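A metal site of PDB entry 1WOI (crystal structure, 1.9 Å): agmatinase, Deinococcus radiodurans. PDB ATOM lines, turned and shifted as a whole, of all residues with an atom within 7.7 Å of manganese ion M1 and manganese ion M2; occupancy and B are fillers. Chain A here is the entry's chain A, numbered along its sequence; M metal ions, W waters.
The side-chain hydroxyl (OG) of Ser 124 sits close to a ring nitrogen (NE2) of His 121 (3.3 Å).
The side-chain carboxylate (OD1) of Asp 231 sits close to the backbone NH (N) of Ala 144, at 3.1 Å.
The backbone NH (N) of Leu 181 sits at hydrogen-bond distance from the backbone carbonyl oxygen (O) of Asp 143, at 3.2 Å.
The side-chain hydroxyl (OG) of Ser 227 is in hydrogen-bond range of a ring nitrogen (NE2) of His 121 (2.9 Å).
The backbone carbonyl oxygen (O) of Leu 142 lies within hydrogen-bond range of the backbone NH (N) of Asp 229, 2.9 Å away.
OE2 of Glu 274 is in hydrogen-bond range of N of His 121 (2.7 Å).
O of His 145 sits at hydrogen-bond distance from NE2 of Gln 141 (3.2 Å).
N of Phe 163 is in hydrogen-bond range of O of Asp 147.
Manganese ion M1 is bound by a ring nitrogen (ND1) of His 121, the side-chain carboxylate (OD2) of Asp 147, the side-chain carboxylate (OD2) of Asp 143, the side-chain carboxylate (OD2) of Asp 229 and water W1.
Manganese ion M1 has five donor atoms within binding distance.
Of the 27 residues printed, 4 come within 4 Å of manganese ion M1.
The nearest printed residue that does not touch manganese ion M1 is His 145 (4.7 Å).
Manganese ion M2 is bound by the side-chain carboxylate (OD2) of Asp 231 (2.2 Å), the side-chain carboxylate (OD1) of Asp 143 (2.3 Å), a ring nitrogen (ND1) of His 145 (2.3 Å), the side-chain carboxylate (OD2) of Asp 229 (2.3 Å), the side-chain carboxylate (OD1) of Asp 231 (2.4 Å) and water W1 (2.6 Å).
Manganese ion M2 has six donor atoms within binding distance.
Within 4 Å of manganese ion M2: Asp 143, His 145, Asp 229 and Asp 231.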
ATOM      1  N   ASP A 120      -9.996 -25.391  22.687  1.00  0.00           N
ATOM      2  CA  ASP A 120     -10.900 -26.541  22.796  1.00  0.00           C
ATOM      3  C   ASP A 120     -11.228 -26.713  24.270  1.00  0.00           C
ATOM      4  O   ASP A 120     -10.649 -26.054  25.126  1.00  0.00           O
ATOM      5  CB  ASP A 120     -10.282 -27.832  22.192  1.00  0.00           C
ATOM      6  CG  ASP A 120      -9.006 -28.278  22.887  1.00  0.00           C
ATOM      7  OD1 ASP A 120      -9.017 -28.463  24.125  1.00  0.00           O
ATOM      8  OD2 ASP A 120      -7.996 -28.491  22.180  1.00  0.00           O
ATOM      9  N   HIS A 121     -12.168 -27.592  24.582  1.00  0.00           N
ATOM     10  CA  HIS A 121     -12.575 -27.767  25.966  1.00  0.00           C
ATOM     11  C   HIS A 121     -11.510 -28.296  26.932  1.00  0.00           C
ATOM     12  O   HIS A 121     -11.695 -28.210  28.147  1.00  0.00           O
ATOM     13  CB  HIS A 121     -13.831 -28.629  26.055  1.00  0.00           C
ATOM     14  CG  HIS A 121     -14.771 -28.193  27.136  1.00  0.00           C
ATOM     15  ND1 HIS A 121     -16.121 -28.455  27.093  1.00  0.00           N
ATOM     16  CD2 HIS A 121     -14.555 -27.500  28.271  1.00  0.00           C
ATOM     17  CE1 HIS A 121     -16.698 -27.928  28.156  1.00  0.00           C
ATOM     18  NE2 HIS A 121     -15.769 -27.345  28.890  1.00  0.00           N
ATOM     19  N   SER A 122     -10.411 -28.829  26.409  1.00  0.00           N
ATOM     20  CA  SER A 122      -9.375 -29.337  27.302  1.00  0.00           C
ATOM     21  C   SER A 122      -8.791 -28.209  28.154  1.00  0.00           C
ATOM     22  O   SER A 122      -8.256 -28.461  29.226  1.00  0.00           O
ATOM     23  CB  SER A 122      -8.244 -30.009  26.515  1.00  0.00           C
ATOM     24  OG  SER A 122      -7.351 -29.060  25.976  1.00  0.00           O
ATOM     25  N   SER A 124     -10.222 -26.085  29.977  1.00  0.00           N
ATOM     26  CA  SER A 124     -10.941 -25.890  31.243  1.00  0.00           C
ATOM     27  C   SER A 124     -10.200 -26.528  32.411  1.00  0.00           C
ATOM     28  O   SER A 124     -10.316 -26.081  33.543  1.00  0.00           O
ATOM     29  CB  SER A 124     -12.352 -26.465  31.156  1.00  0.00           C
ATOM     30  OG  SER A 124     -13.124 -25.773  30.188  1.00  0.00           O
ATOM     31  N   GLN A 141     -21.966 -26.308  33.728  1.00  0.00           N
ATOM     32  CA  GLN A 141     -21.486 -26.588  32.385  1.00  0.00           C
ATOM     33  C   GLN A 141     -22.585 -26.669  31.314  1.00  0.00           C
ATOM     34  O   GLN A 141     -23.533 -27.446  31.459  1.00  0.00           O
ATOM     35  CB  GLN A 141     -20.727 -27.917  32.452  1.00  0.00           C
ATOM     36  CG  GLN A 141     -20.138 -28.475  31.166  1.00  0.00           C
ATOM     37  CD  GLN A 141     -19.650 -29.898  31.350  1.00  0.00           C
ATOM     38  OE1 GLN A 141     -19.610 -30.407  32.478  1.00  0.00           O
ATOM     39  NE2 GLN A 141     -19.265 -30.554  30.254  1.00  0.00           N
ATOM     40  N   LEU A 142     -22.454 -25.862  30.257  1.00  0.00           N
ATOM     41  CA  LEU A 142     -23.392 -25.908  29.142  1.00  0.00           C
ATOM     42  C   LEU A 142     -22.604 -26.727  28.121  1.00  0.00           C
ATOM     43  O   LEU A 142     -21.497 -26.328  27.736  1.00  0.00           O
ATOM     44  CB  LEU A 142     -23.699 -24.519  28.593  1.00  0.00           C
ATOM     45  CG  LEU A 142     -24.494 -23.560  29.489  1.00  0.00           C
ATOM     46  CD1 LEU A 142     -24.957 -22.371  28.668  1.00  0.00           C
ATOM     47  CD2 LEU A 142     -25.697 -24.274  30.065  1.00  0.00           C
ATOM     48  N   ASP A 143     -23.148 -27.850  27.678  1.00  0.00           N
ATOM     49  CA  ASP A 143     -22.373 -28.701  26.771  1.00  0.00           C
ATOM     50  C   ASP A 143     -23.264 -29.803  26.212  1.00  0.00           C
ATOM     51  O   ASP A 143     -24.213 -30.223  26.857  1.00  0.00           O
ATOM     52  CB  ASP A 143     -21.246 -29.350  27.588  1.00  0.00           C
ATOM     53  CG  ASP A 143     -20.050 -29.779  26.756  1.00  0.00           C
ATOM     54  OD1 ASP A 143     -20.240 -30.221  25.600  1.00  0.00           O
ATOM     55  OD2 ASP A 143     -18.928 -29.675  27.287  1.00  0.00           O
ATOM     56  N   ALA A 144     -22.943 -30.264  25.009  1.00  0.00           N
ATOM     57  CA  ALA A 144     -23.679 -31.352  24.412  1.00  0.00           C
ATOM     58  C   ALA A 144     -23.017 -32.625  24.918  1.00  0.00           C
ATOM     59  O   ALA A 144     -23.605 -33.701  24.865  1.00  0.00           O
ATOM     60  CB  ALA A 144     -23.592 -31.293  22.878  1.00  0.00           C
ATOM     61  N   HIS A 145     -21.801 -32.484  25.436  1.00  0.00           N
ATOM     62  CA  HIS A 145     -21.028 -33.621  25.935  1.00  0.00           C
ATOM     63  C   HIS A 145     -20.678 -33.508  27.421  1.00  0.00           C
ATOM     64  O   HIS A 145     -20.613 -32.408  27.979  1.00  0.00           O
ATOM     65  CB  HIS A 145     -19.742 -33.769  25.117  1.00  0.00           C
ATOM     66  CG  HIS A 145     -19.940 -33.611  23.638  1.00  0.00           C
ATOM     67  ND1 HIS A 145     -19.678 -32.431  22.972  1.00  0.00           N
ATOM     68  CD2 HIS A 145     -20.357 -34.484  22.690  1.00  0.00           C
ATOM     69  CE1 HIS A 145     -19.920 -32.587  21.686  1.00  0.00           C
ATOM     70  NE2 HIS A 145     -20.335 -33.822  21.486  1.00  0.00           N
ATOM     71  N   LEU A 146     -20.454 -34.644  28.071  1.00  0.00           N
ATOM     72  CA  LEU A 146     -20.135 -34.663  29.498  1.00  0.00           C
ATOM     73  C   LEU A 146     -18.681 -34.275  29.807  1.00  0.00           C
ATOM     74  O   LEU A 146     -18.413 -33.581  30.789  1.00  0.00           O
ATOM     75  CB  LEU A 146     -20.443 -36.047  30.073  1.00  0.00           C
ATOM     76  CG  LEU A 146     -20.353 -36.187  31.597  1.00  0.00           C
ATOM     77  CD1 LEU A 146     -21.437 -35.334  32.252  1.00  0.00           C
ATOM     78  CD2 LEU A 146     -20.521 -37.653  31.980  1.00  0.00           C
ATOM     79  N   ASP A 147     -17.764 -34.721  28.961  1.00  0.00           N
ATOM     80  CA  ASP A 147     -16.330 -34.449  29.123  1.00  0.00           C
ATOM     81  C   ASP A 147     -15.776 -34.837  30.493  1.00  0.00           C
ATOM     82  O   ASP A 147     -15.024 -34.074  31.111  1.00  0.00           O
ATOM     83  CB  ASP A 147     -16.021 -32.979  28.830  1.00  0.00           C
ATOM     84  CG  ASP A 147     -16.412 -32.567  27.417  1.00  0.00           C
ATOM     85  OD1 ASP A 147     -16.383 -33.415  26.506  1.00  0.00           O
ATOM     86  OD2 ASP A 147     -16.728 -31.379  27.228  1.00  0.00           O
ATOM     87  N   ASN A 159      -9.906 -33.256  24.932  1.00  0.00           N
ATOM     88  CA  ASN A 159     -10.992 -32.380  25.333  1.00  0.00           C
ATOM     89  C   ASN A 159     -12.172 -33.172  25.913  1.00  0.00           C
ATOM     90  O   ASN A 159     -13.203 -32.589  26.248  1.00  0.00           O
ATOM     91  CB  ASN A 159     -11.445 -31.498  24.155  1.00  0.00           C
ATOM     92  CG  ASN A 159     -11.957 -32.295  22.956  1.00  0.00           C
ATOM     93  OD1 ASN A 159     -11.627 -33.472  22.809  1.00  0.00           O
ATOM     94  ND2 ASN A 159     -12.775 -31.670  22.115  1.00  0.00           N
ATOM     95  N   SER A 160     -12.147 -34.406  26.005  1.00  0.00           N
ATOM     96  CA  SER A 160     -13.210 -35.228  26.573  1.00  0.00           C
ATOM     97  C   SER A 160     -12.947 -35.529  28.054  1.00  0.00           C
ATOM     98  O   SER A 160     -13.763 -36.168  28.717  1.00  0.00           O
ATOM     99  CB  SER A 160     -13.330 -36.557  25.807  1.00  0.00           C
ATOM    100  OG  SER A 160     -13.657 -36.351  24.442  1.00  0.00           O
ATOM    101  N   PRO A 162     -11.345 -32.871  30.405  1.00  0.00           N
ATOM    102  CA  PRO A 162     -11.061 -31.743  31.305  1.00  0.00           C
ATOM    103  C   PRO A 162     -11.635 -31.749  32.719  1.00  0.00           C
ATOM    104  O   PRO A 162     -10.931 -31.418  33.671  1.00  0.00           O
ATOM    105  CB  PRO A 162     -11.507 -30.529  30.486  1.00  0.00           C
ATOM    106  CG  PRO A 162     -12.617 -31.075  29.649  1.00  0.00           C
ATOM    107  CD  PRO A 162     -12.063 -32.412  29.201  1.00  0.00           C
ATOM    108  N   PHE A 163     -12.898 -32.123  32.864  1.00  0.00           N
ATOM    109  CA  PHE A 163     -13.490 -32.118  34.194  1.00  0.00           C
ATOM    110  C   PHE A 163     -13.083 -33.314  35.036  1.00  0.00           C
ATOM    111  O   PHE A 163     -13.147 -33.252  36.268  1.00  0.00           O
ATOM    112  CB  PHE A 163     -15.008 -32.002  34.082  1.00  0.00           C
ATOM    113  CG  PHE A 163     -15.439 -30.717  33.452  1.00  0.00           C
ATOM    114  CD1 PHE A 163     -15.985 -30.704  32.177  1.00  0.00           C
ATOM    115  CD2 PHE A 163     -15.207 -29.513  34.104  1.00  0.00           C
ATOM    116  CE1 PHE A 163     -16.287 -29.495  31.554  1.00  0.00           C
ATOM    117  CE2 PHE A 163     -15.500 -28.291  33.487  1.00  0.00           C
ATOM    118  CZ  PHE A 163     -16.036 -28.288  32.203  1.00  0.00           C
ATOM    119  N   LEU A 181     -26.772 -32.081  27.511  1.00  0.00           N
ATOM    120  CA  LEU A 181     -26.318 -33.362  26.972  1.00  0.00           C
ATOM    121  C   LEU A 181     -27.287 -34.040  26.007  1.00  0.00           C
ATOM    122  O   LEU A 181     -28.491 -34.093  26.246  1.00  0.00           O
ATOM    123  CB  LEU A 181     -26.010 -34.330  28.131  1.00  0.00           C
ATOM    124  CG  LEU A 181     -24.939 -33.866  29.118  1.00  0.00           C
ATOM    125  CD1 LEU A 181     -24.658 -34.996  30.110  1.00  0.00           C
ATOM    126  CD2 LEU A 181     -23.660 -33.503  28.371  1.00  0.00           C
ATOM    127  N   SER A 227     -18.750 -22.848  32.611  1.00  0.00           N
ATOM    128  CA  SER A 227     -18.009 -23.386  31.482  1.00  0.00           C
ATOM    129  C   SER A 227     -19.020 -23.511  30.356  1.00  0.00           C
ATOM    130  O   SER A 227     -19.906 -24.360  30.393  1.00  0.00           O
ATOM    131  CB  SER A 227     -17.414 -24.754  31.783  1.00  0.00           C
ATOM    132  OG  SER A 227     -16.697 -25.215  30.650  1.00  0.00           O
ATOM    133  N   VAL A 228     -18.885 -22.663  29.350  1.00  0.00           N
ATOM    134  CA  VAL A 228     -19.798 -22.697  28.218  1.00  0.00           C
ATOM    135  C   VAL A 228     -19.145 -23.275  26.977  1.00  0.00           C
ATOM    136  O   VAL A 228     -18.245 -22.664  26.401  1.00  0.00           O
ATOM    137  CB  VAL A 228     -20.332 -21.290  27.889  1.00  0.00           C
ATOM    138  CG1 VAL A 228     -21.338 -21.371  26.720  1.00  0.00           C
ATOM    139  CG2 VAL A 228     -20.993 -20.674  29.122  1.00  0.00           C
ATOM    140  N   ASP A 229     -19.599 -24.454  26.574  1.00  0.00           N
ATOM    141  CA  ASP A 229     -19.105 -25.100  25.364  1.00  0.00           C
ATOM    142  C   ASP A 229     -20.152 -24.707  24.322  1.00  0.00           C
ATOM    143  O   ASP A 229     -21.337 -25.043  24.477  1.00  0.00           O
ATOM    144  CB  ASP A 229     -19.091 -26.613  25.532  1.00  0.00           C
ATOM    145  CG  ASP A 229     -18.566 -27.339  24.304  1.00  0.00           C
ATOM    146  OD1 ASP A 229     -18.747 -26.859  23.175  1.00  0.00           O
ATOM    147  OD2 ASP A 229     -17.970 -28.419  24.486  1.00  0.00           O
ATOM    148  N   VAL A 230     -19.743 -24.008  23.275  1.00  0.00           N
ATOM    149  CA  VAL A 230     -20.716 -23.582  22.275  1.00  0.00           C
ATOM    150  C   VAL A 230     -21.517 -24.702  21.634  1.00  0.00           C
ATOM    151  O   VAL A 230     -22.610 -24.454  21.120  1.00  0.00           O
ATOM    152  CB  VAL A 230     -20.059 -22.711  21.159  1.00  0.00           C
ATOM    153  CG1 VAL A 230     -19.302 -21.542  21.776  1.00  0.00           C
ATOM    154  CG2 VAL A 230     -19.120 -23.561  20.298  1.00  0.00           C
ATOM    155  N   ASP A 231     -21.008 -25.944  21.659  1.00  0.00           N
ATOM    156  CA  ASP A 231     -21.795 -27.007  21.033  1.00  0.00           C
ATOM    157  C   ASP A 231     -22.997 -27.398  21.879  1.00  0.00           C
ATOM    158  O   ASP A 231     -23.810 -28.237  21.465  1.00  0.00           O
ATOM    159  CB  ASP A 231     -20.946 -28.239  20.648  1.00  0.00           C
ATOM    160  CG  ASP A 231     -20.323 -28.951  21.832  1.00  0.00           C
ATOM    161  OD1 ASP A 231     -20.952 -29.022  22.916  1.00  0.00           O
ATOM    162  OD2 ASP A 231     -19.191 -29.450  21.659  1.00  0.00           O
ATOM    163  N   GLY A 232     -23.138 -26.761  23.043  1.00  0.00           N
ATOM    164  CA  GLY A 232     -24.316 -27.017  23.864  1.00  0.00           C
ATOM    165  C   GLY A 232     -25.504 -26.382  23.143  1.00  0.00           C
ATOM    166  O   GLY A 232     -26.644 -26.828  23.274  1.00  0.00           O
ATOM    167  N   THR A 241     -18.537 -25.090  15.288  1.00  0.00           N
ATOM    168  CA  THR A 241     -17.941 -25.889  16.372  1.00  0.00           C
ATOM    169  C   THR A 241     -17.540 -27.234  15.774  1.00  0.00           C
ATOM    170  O   THR A 241     -18.125 -27.690  14.799  1.00  0.00           O
ATOM    171  CB  THR A 241     -18.946 -26.082  17.545  1.00  0.00           C
ATOM    172  OG1 THR A 241     -18.252 -26.577  18.698  1.00  0.00           O
ATOM    173  CG2 THR A 241     -20.049 -27.056  17.168  1.00  0.00           C
ATOM    174  N   SER A 243     -17.733 -30.559  16.826  1.00  0.00           N
ATOM    175  CA  SER A 243     -18.640 -31.699  16.881  1.00  0.00           C
ATOM    176  C   SER A 243     -20.077 -31.369  17.247  1.00  0.00           C
ATOM    177  O   SER A 243     -20.504 -31.608  18.378  1.00  0.00           O
ATOM    178  CB  SER A 243     -18.087 -32.709  17.885  1.00  0.00           C
ATOM    179  OG  SER A 243     -16.696 -32.896  17.661  1.00  0.00           O
ATOM    180  N   PRO A 244     -20.835 -30.818  16.288  1.00  0.00           N
ATOM    181  CA  PRO A 244     -22.240 -30.453  16.536  1.00  0.00           C
ATOM    182  C   PRO A 244     -23.164 -31.644  16.771  1.00  0.00           C
ATOM    183  O   PRO A 244     -22.947 -32.734  16.238  1.00  0.00           O
ATOM    184  CB  PRO A 244     -22.610 -29.674  15.275  1.00  0.00           C
ATOM    185  CG  PRO A 244     -21.775 -30.326  14.209  1.00  0.00           C
ATOM    186  CD  PRO A 244     -20.431 -30.486  14.910  1.00  0.00           C
ATOM    187  N   VAL A 273     -15.628 -22.015  25.350  1.00  0.00           N
ATOM    188  CA  VAL A 273     -14.799 -22.925  24.562  1.00  0.00           C
ATOM    189  C   VAL A 273     -15.450 -23.588  23.345  1.00  0.00           C
ATOM    190  O   VAL A 273     -16.660 -23.535  23.175  1.00  0.00           O
ATOM    191  CB  VAL A 273     -14.238 -24.047  25.466  1.00  0.00           C
ATOM    192  CG1 VAL A 273     -13.466 -23.446  26.615  1.00  0.00           C
ATOM    193  CG2 VAL A 273     -15.385 -24.928  25.978  1.00  0.00           C
ATOM    194  N   GLU A 274     -14.596 -24.188  22.523  1.00  0.00           N
ATOM    195  CA  GLU A 274     -14.984 -24.931  21.313  1.00  0.00           C
ATOM    196  C   GLU A 274     -15.558 -24.124  20.140  1.00  0.00           C
ATOM    197  O   GLU A 274     -16.105 -24.701  19.198  1.00  0.00           O
ATOM    198  CB  GLU A 274     -15.932 -26.071  21.676  1.00  0.00           C
ATOM    199  CG  GLU A 274     -15.327 -27.191  22.541  1.00  0.00           C
ATOM    200  CD  GLU A 274     -14.296 -28.071  21.806  1.00  0.00           C
ATOM    201  OE1 GLU A 274     -14.302 -28.109  20.559  1.00  0.00           O
ATOM    202  OE2 GLU A 274     -13.493 -28.741  22.484  1.00  0.00           O
HETATM  203 MN    MN M   1     -17.223 -29.773  26.026  1.00  0.00          MN
HETATM  204 MN    MN M   2     -19.042 -30.330  23.696  1.00  0.00          MN
HETATM  205  O   HOH W   1     -16.724 -31.268  24.241  1.00  0.00           O
